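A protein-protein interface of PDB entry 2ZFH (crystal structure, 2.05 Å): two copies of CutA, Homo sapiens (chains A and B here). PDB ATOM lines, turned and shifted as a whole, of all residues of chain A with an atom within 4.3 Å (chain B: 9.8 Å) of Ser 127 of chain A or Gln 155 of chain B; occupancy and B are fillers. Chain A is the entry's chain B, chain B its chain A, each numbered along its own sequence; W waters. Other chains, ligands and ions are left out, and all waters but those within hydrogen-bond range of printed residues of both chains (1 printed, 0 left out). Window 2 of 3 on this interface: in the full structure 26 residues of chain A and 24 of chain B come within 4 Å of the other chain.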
ATOM      1  N   GLY A  66      15.113  26.979  39.918  1.00  0.00           N
ATOM      2  CA  GLY A  66      14.434  27.638  38.815  1.00  0.00           C
ATOM      3  C   GLY A  66      14.854  29.051  38.447  1.00  0.00           C
ATOM      4  O   GLY A  66      14.274  29.624  37.526  1.00  0.00           O
ATOM      5  N   SER A  67      15.851  29.619  39.123  1.00  0.00           N
ATOM      6  CA  SER A  67      16.259  30.988  38.816  1.00  0.00           C
ATOM      7  C   SER A  67      17.078  31.045  37.527  1.00  0.00           C
ATOM      8  O   SER A  67      17.222  32.104  36.908  1.00  0.00           O
ATOM      9  CB  SER A  67      17.028  31.600  39.988  1.00  0.00           C
ATOM     10  OG  SER A  67      18.222  30.892  40.266  1.00  0.00           O
ATOM     11  N   VAL A  68      17.609  29.896  37.124  1.00  0.00           N
ATOM     12  CA  VAL A  68      18.353  29.804  35.878  1.00  0.00           C
ATOM     13  C   VAL A  68      17.543  28.864  34.984  1.00  0.00           C
ATOM     14  O   VAL A  68      16.942  27.895  35.464  1.00  0.00           O
ATOM     15  CB  VAL A  68      19.774  29.218  36.081  1.00  0.00           C
ATOM     16  CG1 VAL A  68      20.401  28.892  34.737  1.00  0.00           C
ATOM     17  CG2 VAL A  68      20.659  30.219  36.807  1.00  0.00           C
ATOM     18  N   SER A  69      17.511  29.154  33.691  1.00  0.00           N
ATOM     19  CA  SER A  69      16.781  28.317  32.756  1.00  0.00           C
ATOM     20  C   SER A  69      17.651  27.897  31.594  1.00  0.00           C
ATOM     21  O   SER A  69      18.670  28.519  31.308  1.00  0.00           O
ATOM     22  CB  SER A  69      15.559  29.058  32.203  1.00  0.00           C
ATOM     23  OG  SER A  69      14.537  29.161  33.177  1.00  0.00           O
ATOM     24  N   THR A 125      20.715  31.001  30.912  1.00  0.00           N
ATOM     25  CA  THR A 125      20.552  32.363  31.377  1.00  0.00           C
ATOM     26  C   THR A 125      19.599  32.419  32.571  1.00  0.00           C
ATOM     27  O   THR A 125      18.983  31.415  32.931  1.00  0.00           O
ATOM     28  CB  THR A 125      19.995  33.245  30.244  1.00  0.00           C
ATOM     29  OG1 THR A 125      19.918  34.601  30.692  1.00  0.00           O
ATOM     30  CG2 THR A 125      18.598  32.772  29.831  1.00  0.00           C
ATOM     31  N   GLN A 126      19.504  33.588  33.200  1.00  0.00           N
ATOM     32  CA  GLN A 126      18.595  33.774  34.328  1.00  0.00           C
ATOM     33  C   GLN A 126      17.182  33.607  33.782  1.00  0.00           C
ATOM     34  O   GLN A 126      16.883  34.084  32.692  1.00  0.00           O
ATOM     35  CB  GLN A 126      18.712  35.189  34.906  1.00  0.00           C
ATOM     36  CG  GLN A 126      19.871  35.438  35.863  1.00  0.00           C
ATOM     37  CD  GLN A 126      19.900  36.887  36.335  1.00  0.00           C
ATOM     38  OE1 GLN A 126      20.721  37.684  35.881  1.00  0.00           O
ATOM     39  NE2 GLN A 126      18.981  37.236  37.228  1.00  0.00           N
ATOM     40  N   SER A 127      16.317  32.944  34.540  1.00  0.00           N
ATOM     41  CA  SER A 127      14.938  32.741  34.116  1.00  0.00           C
ATOM     42  C   SER A 127      14.241  34.080  33.882  1.00  0.00           C
ATOM     43  O   SER A 127      13.399  34.213  32.994  1.00  0.00           O
ATOM     44  CB  SER A 127      14.178  31.949  35.180  1.00  0.00           C
ATOM     45  OG  SER A 127      14.783  30.685  35.377  1.00  0.00           O
ATOM     46  N   SER A 128      14.595  35.076  34.687  1.00  0.00           N
ATOM     47  CA  SER A 128      13.987  36.391  34.563  1.00  0.00           C
ATOM     48  C   SER A 128      14.321  37.060  33.226  1.00  0.00           C
ATOM     49  O   SER A 128      13.601  37.955  32.773  1.00  0.00           O
ATOM     50  CB  SER A 128      14.441  37.279  35.719  1.00  0.00           C
ATOM     51  OG  SER A 128      15.846  37.445  35.693  1.00  0.00           O
ATOM     52  N   LEU A 129      15.398  36.618  32.585  1.00  0.00           N
ATOM     53  CA  LEU A 129      15.799  37.199  31.307  1.00  0.00           C
ATOM     54  C   LEU A 129      15.256  36.484  30.072  1.00  0.00           C
ATOM     55  O   LEU A 129      15.470  36.941  28.952  1.00  0.00           O
ATOM     56  CB  LEU A 129      17.329  37.267  31.219  1.00  0.00           C
ATOM     57  CG  LEU A 129      18.004  38.281  32.157  1.00  0.00           C
ATOM     58  CD1 LEU A 129      19.505  38.067  32.172  1.00  0.00           C
ATOM     59  CD2 LEU A 129      17.664  39.705  31.706  1.00  0.00           C
ATOM     60  N   VAL A 130      14.547  35.375  30.259  1.00  0.00           N
ATOM     61  CA  VAL A 130      14.033  34.635  29.106  1.00  0.00           C
ATOM     62  C   VAL A 130      13.147  35.494  28.213  1.00  0.00           C
ATOM     63  O   VAL A 130      13.224  35.398  26.992  1.00  0.00           O
ATOM     64  CB  VAL A 130      13.275  33.357  29.544  1.00  0.00           C
ATOM     65  CG1 VAL A 130      12.543  32.733  28.360  1.00  0.00           C
ATOM     66  CG2 VAL A 130      14.266  32.354  30.105  1.00  0.00           C
ATOM     67  N   PRO A 131      12.285  36.342  28.807  1.00  0.00           N
ATOM     68  CA  PRO A 131      11.421  37.189  27.977  1.00  0.00           C
ATOM     69  C   PRO A 131      12.234  38.141  27.080  1.00  0.00           C
ATOM     70  O   PRO A 131      11.980  38.251  25.876  1.00  0.00           O
ATOM     71  CB  PRO A 131      10.574  37.919  29.011  1.00  0.00           C
ATOM     72  CG  PRO A 131      10.444  36.888  30.102  1.00  0.00           C
ATOM     73  CD  PRO A 131      11.861  36.395  30.218  1.00  0.00           C
ATOM     74  N   ILE A 149      12.014  27.750  23.469  1.00  0.00           N
ATOM     75  CA  ILE A 149      11.414  27.085  24.617  1.00  0.00           C
ATOM     76  C   ILE A 149      12.445  27.058  25.729  1.00  0.00           C
ATOM     77  O   ILE A 149      13.635  26.853  25.484  1.00  0.00           O
ATOM     78  CB  ILE A 149      10.966  25.636  24.291  1.00  0.00           C
ATOM     79  CG1 ILE A 149      12.170  24.773  23.924  1.00  0.00           C
ATOM     80  CG2 ILE A 149       9.965  25.644  23.143  1.00  0.00           C
ATOM     81  CD1 ILE A 149      11.812  23.319  23.727  1.00  0.00           C
ATOM     82  N   ALA A 150      11.991  27.286  26.954  1.00  0.00           N
ATOM     83  CA  ALA A 150      12.892  27.302  28.096  1.00  0.00           C
ATOM     84  C   ALA A 150      12.430  26.356  29.197  1.00  0.00           C
ATOM     85  O   ALA A 150      11.241  26.284  29.530  1.00  0.00           O
ATOM     86  CB  ALA A 150      13.015  28.723  28.638  1.00  0.00           C
ATOM     87  N   GLY B  62      -1.404  34.616  26.009  1.00  0.00           N
ATOM     88  CA  GLY B  62      -0.344  34.189  26.903  1.00  0.00           C
ATOM     89  C   GLY B  62       0.055  32.743  26.690  1.00  0.00           C
ATOM     90  O   GLY B  62      -0.101  32.193  25.598  1.00  0.00           O
ATOM     91  N   TYR B  63       0.584  32.129  27.741  1.00  0.00           N
ATOM     92  CA  TYR B  63       1.016  30.739  27.701  1.00  0.00           C
ATOM     93  C   TYR B  63       0.873  30.169  29.103  1.00  0.00           C
ATOM     94  O   TYR B  63       1.272  30.801  30.072  1.00  0.00           O
ATOM     95  CB  TYR B  63       2.483  30.641  27.246  1.00  0.00           C
ATOM     96  CG  TYR B  63       3.078  29.253  27.400  1.00  0.00           C
ATOM     97  CD1 TYR B  63       2.639  28.190  26.610  1.00  0.00           C
ATOM     98  CD2 TYR B  63       4.048  28.995  28.370  1.00  0.00           C
ATOM     99  CE1 TYR B  63       3.145  26.902  26.787  1.00  0.00           C
ATOM    100  CE2 TYR B  63       4.564  27.713  28.556  1.00  0.00           C
ATOM    101  CZ  TYR B  63       4.106  26.669  27.762  1.00  0.00           C
ATOM    102  OH  TYR B  63       4.595  25.396  27.962  1.00  0.00           O
ATOM    103  N   VAL B  64       0.286  28.986  29.212  1.00  0.00           N
ATOM    104  CA  VAL B  64       0.115  28.339  30.506  1.00  0.00           C
ATOM    105  C   VAL B  64       1.376  27.537  30.775  1.00  0.00           C
ATOM    106  O   VAL B  64       1.662  26.569  30.081  1.00  0.00           O
ATOM    107  CB  VAL B  64      -1.115  27.404  30.498  1.00  0.00           C
ATOM    108  CG1 VAL B  64      -1.241  26.693  31.831  1.00  0.00           C
ATOM    109  CG2 VAL B  64      -2.382  28.222  30.205  1.00  0.00           C
ATOM    110  N   PRO B  65       2.154  27.935  31.795  1.00  0.00           N
ATOM    111  CA  PRO B  65       3.387  27.203  32.093  1.00  0.00           C
ATOM    112  C   PRO B  65       3.162  25.710  32.257  1.00  0.00           C
ATOM    113  O   PRO B  65       2.221  25.287  32.920  1.00  0.00           O
ATOM    114  CB  PRO B  65       3.881  27.874  33.368  1.00  0.00           C
ATOM    115  CG  PRO B  65       3.399  29.293  33.191  1.00  0.00           C
ATOM    116  CD  PRO B  65       1.984  29.070  32.715  1.00  0.00           C
ATOM    117  N   GLY B  66       4.022  24.921  31.620  1.00  0.00           N
ATOM    118  CA  GLY B  66       3.926  23.474  31.707  1.00  0.00           C
ATOM    119  C   GLY B  66       2.930  22.811  30.771  1.00  0.00           C
ATOM    120  O   GLY B  66       2.859  21.586  30.734  1.00  0.00           O
ATOM    121  N   SER B  67       2.167  23.592  30.012  1.00  0.00           N
ATOM    122  CA  SER B  67       1.179  23.003  29.105  1.00  0.00           C
ATOM    123  C   SER B  67       1.836  22.322  27.902  1.00  0.00           C
ATOM    124  O   SER B  67       1.248  21.426  27.293  1.00  0.00           O
ATOM    125  CB  SER B  67       0.151  24.055  28.662  1.00  0.00           C
ATOM    126  OG  SER B  67       0.755  25.161  28.023  1.00  0.00           O
ATOM    127  N   VAL B  68       3.057  22.740  27.575  1.00  0.00           N
ATOM    128  CA  VAL B  68       3.821  22.128  26.491  1.00  0.00           C
ATOM    129  C   VAL B  68       5.065  21.480  27.105  1.00  0.00           C
ATOM    130  O   VAL B  68       5.626  21.982  28.087  1.00  0.00           O
ATOM    131  CB  VAL B  68       4.268  23.164  25.430  1.00  0.00           C
ATOM    132  CG1 VAL B  68       5.290  22.538  24.478  1.00  0.00           C
ATOM    133  CG2 VAL B  68       3.065  23.655  24.634  1.00  0.00           C
ATOM    134  N   SER B  69       5.482  20.354  26.534  1.00  0.00           N
ATOM    135  CA  SER B  69       6.658  19.641  27.016  1.00  0.00           C
ATOM    136  C   SER B  69       7.619  19.255  25.900  1.00  0.00           C
ATOM    137  O   SER B  69       7.265  19.255  24.723  1.00  0.00           O
ATOM    138  CB  SER B  69       6.250  18.369  27.768  1.00  0.00           C
ATOM    139  OG  SER B  69       5.614  18.680  28.993  1.00  0.00           O
ATOM    140  N   ALA B  70       8.848  18.937  26.292  1.00  0.00           N
ATOM    141  CA  ALA B  70       9.877  18.503  25.364  1.00  0.00           C
ATOM    142  C   ALA B  70      10.197  17.097  25.848  1.00  0.00           C
ATOM    143  O   ALA B  70      10.537  16.900  27.008  1.00  0.00           O
ATOM    144  CB  ALA B  70      11.114  19.399  25.472  1.00  0.00           C
ATOM    145  N   LYS B 124       8.593  18.084  20.672  1.00  0.00           N
ATOM    146  CA  LYS B 124       7.793  19.147  21.259  1.00  0.00           C
ATOM    147  C   LYS B 124       6.319  18.865  21.055  1.00  0.00           C
ATOM    148  O   LYS B 124       5.838  18.780  19.925  1.00  0.00           O
ATOM    149  CB  LYS B 124       8.132  20.506  20.636  1.00  0.00           C
ATOM    150  CG  LYS B 124       9.427  21.146  21.127  1.00  0.00           C
ATOM    151  CD  LYS B 124      10.666  20.387  20.689  1.00  0.00           C
ATOM    152  CE  LYS B 124      10.841  20.389  19.172  1.00  0.00           C
ATOM    153  NZ  LYS B 124      10.935  21.771  18.628  1.00  0.00           N
ATOM    154  N   LEU B 151      10.160  16.864  29.745  1.00  0.00           N
ATOM    155  CA  LEU B 151      10.403  18.003  30.627  1.00  0.00           C
ATOM    156  C   LEU B 151       9.452  19.141  30.265  1.00  0.00           C
ATOM    157  O   LEU B 151       9.295  19.478  29.098  1.00  0.00           O
ATOM    158  CB  LEU B 151      11.853  18.474  30.486  1.00  0.00           C
ATOM    159  CG  LEU B 151      12.982  17.501  30.849  1.00  0.00           C
ATOM    160  CD1 LEU B 151      13.093  16.389  29.806  1.00  0.00           C
ATOM    161  CD2 LEU B 151      14.291  18.277  30.915  1.00  0.00           C
ATOM    162  N   PRO B 152       8.814  19.757  31.269  1.00  0.00           N
ATOM    163  CA  PRO B 152       7.874  20.856  31.023  1.00  0.00           C
ATOM    164  C   PRO B 152       8.515  22.175  30.615  1.00  0.00           C
ATOM    165  O   PRO B 152       9.520  22.606  31.184  1.00  0.00           O
ATOM    166  CB  PRO B 152       7.129  20.966  32.349  1.00  0.00           C
ATOM    167  CG  PRO B 152       8.202  20.687  33.328  1.00  0.00           C
ATOM    168  CD  PRO B 152       8.938  19.496  32.714  1.00  0.00           C
ATOM    169  N   VAL B 153       7.919  22.805  29.612  1.00  0.00           N
ATOM    170  CA  VAL B 153       8.379  24.085  29.110  1.00  0.00           C
ATOM    171  C   VAL B 153       7.665  25.143  29.946  1.00  0.00           C
ATOM    172  O   VAL B 153       6.440  25.168  30.004  1.00  0.00           O
ATOM    173  CB  VAL B 153       8.022  24.244  27.603  1.00  0.00           C
ATOM    174  CG1 VAL B 153       8.360  25.645  27.129  1.00  0.00           C
ATOM    175  CG2 VAL B 153       8.789  23.201  26.774  1.00  0.00           C
ATOM    176  N   GLU B 154       8.435  26.001  30.602  1.00  0.00           N
ATOM    177  CA  GLU B 154       7.870  27.042  31.458  1.00  0.00           C
ATOM    178  C   GLU B 154       7.684  28.387  30.778  1.00  0.00           C
ATOM    179  O   GLU B 154       6.743  29.110  31.087  1.00  0.00           O
ATOM    180  CB  GLU B 154       8.751  27.245  32.690  1.00  0.00           C
ATOM    181  CG  GLU B 154       8.796  26.055  33.625  1.00  0.00           C
ATOM    182  CD  GLU B 154       7.429  25.705  34.164  1.00  0.00           C
ATOM    183  OE1 GLU B 154       6.709  26.636  34.577  1.00  0.00           O
ATOM    184  OE2 GLU B 154       7.073  24.508  34.182  1.00  0.00           O
ATOM    185  N   GLN B 155       8.603  28.729  29.884  1.00  0.00           N
ATOM    186  CA  GLN B 155       8.570  29.992  29.160  1.00  0.00           C
ATOM    187  C   GLN B 155       8.953  29.737  27.704  1.00  0.00           C
ATOM    188  O   GLN B 155       9.205  28.596  27.309  1.00  0.00           O
ATOM    189  CB  GLN B 155       9.576  30.992  29.752  1.00  0.00           C
ATOM    190  CG  GLN B 155       9.399  31.337  31.223  1.00  0.00           C
ATOM    191  CD  GLN B 155      10.357  32.444  31.674  1.00  0.00           C
ATOM    192  OE1 GLN B 155      10.160  33.610  31.364  1.00  0.00           O
ATOM    193  NE2 GLN B 155      11.404  32.070  32.391  1.00  0.00           N
ATOM    194  N   GLY B 156       9.009  30.809  26.916  1.00  0.00           N
ATOM    195  CA  GLY B 156       9.381  30.682  25.516  1.00  0.00           C
ATOM    196  C   GLY B 156       8.660  31.659  24.607  1.00  0.00           C
ATOM    197  O   GLY B 156       8.091  32.645  25.070  1.00  0.00           O
ATOM    198  N   ASN B 157       8.681  31.385  23.306  1.00  0.00           N
ATOM    199  CA  ASN B 157       8.026  32.247  22.331  1.00  0.00           C
ATOM    200  C   ASN B 157       6.552  31.850  22.227  1.00  0.00           C
ATOM    201  O   ASN B 157       6.204  30.815  21.658  1.00  0.00           O
ATOM    202  CB  ASN B 157       8.731  32.122  20.973  1.00  0.00           C
ATOM    203  CG  ASN B 157       8.275  33.178  19.978  1.00  0.00           C
ATOM    204  OD1 ASN B 157       7.777  34.232  20.364  1.00  0.00           O
ATOM    205  ND2 ASN B 157       8.459  32.903  18.693  1.00  0.00           N
ATOM    206  N   PHE B 158       5.691  32.685  22.791  1.00  0.00           N
ATOM    207  CA  PHE B 158       4.256  32.431  22.802  1.00  0.00           C
ATOM    208  C   PHE B 158       3.637  32.005  21.468  1.00  0.00           C
ATOM    209  O   PHE B 158       2.887  31.038  21.431  1.00  0.00           O
ATOM    210  CB  PHE B 158       3.530  33.643  23.398  1.00  0.00           C
ATOM    211  CG  PHE B 158       3.814  33.849  24.878  1.00  0.00           C
ATOM    212  CD1 PHE B 158       4.804  33.100  25.528  1.00  0.00           C
ATOM    213  CD2 PHE B 158       3.093  34.785  25.620  1.00  0.00           C
ATOM    214  CE1 PHE B 158       5.068  33.278  26.885  1.00  0.00           C
ATOM    215  CE2 PHE B 158       3.349  34.973  26.987  1.00  0.00           C
ATOM    216  CZ  PHE B 158       4.336  34.221  27.619  1.00  0.00           C
ATOM    217  N   PRO B 159       3.928  32.717  20.362  1.00  0.00           N
ATOM    218  CA  PRO B 159       3.335  32.286  19.086  1.00  0.00           C
ATOM    219  C   PRO B 159       3.776  30.865  18.688  1.00  0.00           C
ATOM    220  O   PRO B 159       3.004  30.102  18.103  1.00  0.00           O
ATOM    221  CB  PRO B 159       3.806  33.361  18.098  1.00  0.00           C
ATOM    222  CG  PRO B 159       5.058  33.898  18.730  1.00  0.00           C
ATOM    223  CD  PRO B 159       4.683  33.970  20.187  1.00  0.00           C
ATOM    224  N   TYR B 160       5.015  30.510  19.019  1.00  0.00           N
ATOM    225  CA  TYR B 160       5.532  29.178  18.724  1.00  0.00           C
ATOM    226  C   TYR B 160       4.796  28.149  19.580  1.00  0.00           C
ATOM    227  O   TYR B 160       4.299  27.136  19.071  1.00  0.00           O
ATOM    228  CB  TYR B 160       7.028  29.103  19.026  1.00  0.00           C
ATOM    229  CG  TYR B 160       7.614  27.720  18.826  1.00  0.00           C
ATOM    230  CD1 TYR B 160       7.845  27.215  17.545  1.00  0.00           C
ATOM    231  CD2 TYR B 160       7.923  26.912  19.917  1.00  0.00           C
ATOM    232  CE1 TYR B 160       8.372  25.943  17.355  1.00  0.00           C
ATOM    233  CE2 TYR B 160       8.447  25.636  19.742  1.00  0.00           C
ATOM    234  CZ  TYR B 160       8.673  25.159  18.458  1.00  0.00           C
ATOM    235  OH  TYR B 160       9.227  23.911  18.284  1.00  0.00           O
ATOM    236  N   LEU B 161       4.735  28.417  20.886  1.00  0.00           N
ATOM    237  CA  LEU B 161       4.064  27.523  21.821  1.00  0.00           C
ATOM    238  C   LEU B 161       2.591  27.382  21.455  1.00  0.00           C
ATOM    239  O   LEU B 161       2.009  26.302  21.588  1.00  0.00           O
ATOM    240  CB  LEU B 161       4.212  28.053  23.249  1.00  0.00           C
ATOM    241  CG  LEU B 161       5.656  28.003  23.757  1.00  0.00           C
ATOM    242  CD1 LEU B 161       5.839  28.878  24.988  1.00  0.00           C
ATOM    243  CD2 LEU B 161       6.022  26.558  24.035  1.00  0.00           C
ATOM    244  N   GLN B 162       1.990  28.477  20.995  1.00  0.00           N
ATOM    245  CA  GLN B 162       0.588  28.470  20.588  1.00  0.00           C
ATOM    246  C   GLN B 162       0.434  27.547  19.374  1.00  0.00           C
ATOM    247  O   GLN B 162      -0.551  26.809  19.256  1.00  0.00           O
ATOM    248  CB  GLN B 162       0.136  29.881  20.207  1.00  0.00           C
ATOM    249  CG  GLN B 162      -1.354  29.982  19.928  1.00  0.00           C
ATOM    250  CD  GLN B 162      -1.753  31.301  19.290  1.00  0.00           C
ATOM    251  OE1 GLN B 162      -2.930  31.666  19.291  1.00  0.00           O
ATOM    252  NE2 GLN B 162      -0.780  32.016  18.729  1.00  0.00           N
HETATM  253  O   HOH W   1      11.961  29.275  32.928  1.00  0.00           O
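Positions printed for both chains: 66, 67, 68 and 69.
Of the 9 pairs that touch across the chains among the printed residues, none has its exchanged pair printed and touching as well.
Among the printed residues, pairs that only touch across the chains: Val 130 of chain A with Gln 155 of chain B, Pro 131 of chain A with Gln 155 of chain B, Ile 149 of chain A with Val 153 of chain B, Ile 149 of chain A with Gln 155 of chain B, Ile 149 of chain A with Tyr 160 of chain B and Ala 150 of chain A with Val 153 of chain B.
Ser 127 of chain A touches just one residue of chain B: Gln 155.
No residue of chain B comes within 4 Å of Ser 128 of chain A.
Of chain B, only Gln 155 comes within 4 Å of Val 130 of chain A.
Of the printed residues of chain B, Pro 131 of chain A touches Gln 155.
Of the printed residues of chain B, Ile 149 of chain A touches Val 153, Gln 155 and Tyr 160.
Of chain B, only Val 153, Glu 154 and Gln 155 come within 4 Å of Ala 150 of chain A.
Of the printed residues of chain A, Val 153 of chain B touches Ile 149 (3.9 Å) and Ala 150 (3.6 Å).
Of the printed residues of chain A, Glu 154 of chain B touches Ala 150.
Gln 155 of chain B touches just these residues of chain A: Ser 127, Val 130, Pro 131, Ile 149 and Ala 150.
Printed residues of chain A within 4 Å of Tyr 160 of chain B: Ile 149.
The nearest residue of chain B that does not touch Ser 127 of chain A is Glu 154 of chain B (7.4 Å).
The backbone NH (N) of Val 153 of chain B lies within hydrogen-bond range of the backbone carbonyl oxygen (O) of Val 68 of chain B.
The side-chain hydroxyl of Tyr 63 of chain B is in hydrogen-bond range of the backbone carbonyl oxygen of Val 153 of chain B, at 2.8 Å.
The backbone carbonyl oxygen (O) of Gly 66 of chain A is in hydrogen-bond range of the side-chain hydroxyl (OG) of Ser 127 of chain A (2.5 Å).
The backbone NH (N) of Val 68 of chain A lies close to the side-chain hydroxyl (OG) of Ser 127 of chain A.
The side-chain amino group (NZ) of Lys 124 of chain B sits at hydrogen-bond distance from the side-chain hydroxyl (OH) of Tyr 160 of chain B (2.8 Å).
The side-chain hydroxyl of Ser 69 of chain A lies within hydrogen-bond range of the side-chain hydroxyl of Ser 127 of chain A (2.7 Å).
O of Ala 150 of chain A is in hydrogen-bond range of N of Glu 154 of chain B, at 3.0 Å.
The backbone carbonyl oxygen (O) of Ser 127 of chain A is in hydrogen-bond range of the side-chain amide nitrogen (NE2) of Gln 155 of chain B, at 3.0 Å.
The backbone NH (N) of Ala 150 of chain A is in hydrogen-bond range of the backbone carbonyl oxygen (O) of Gln 155 of chain B (3.1 Å).
Water W1 bridges OG of Ser 69 of chain A (2.6 Å) and NE2 of Gln 155 of chain B (2.9 Å).
Hydrophobic or aromatic side chains of chain A that line the printed part of chain B: Val 130, Pro 131 and Ile 149.
Of the 22 printed residues of chain B, 4 touch a printed residue of chain A.
Printed residues of chain B that touch a printed residue of chain A: Val 153, Glu 154, Gln 155 and Tyr 160.
Among the printed residues, no Asp or Glu carboxylate lies within 4 Å of a Lys or Arg side-chain nitrogen of the other chain.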
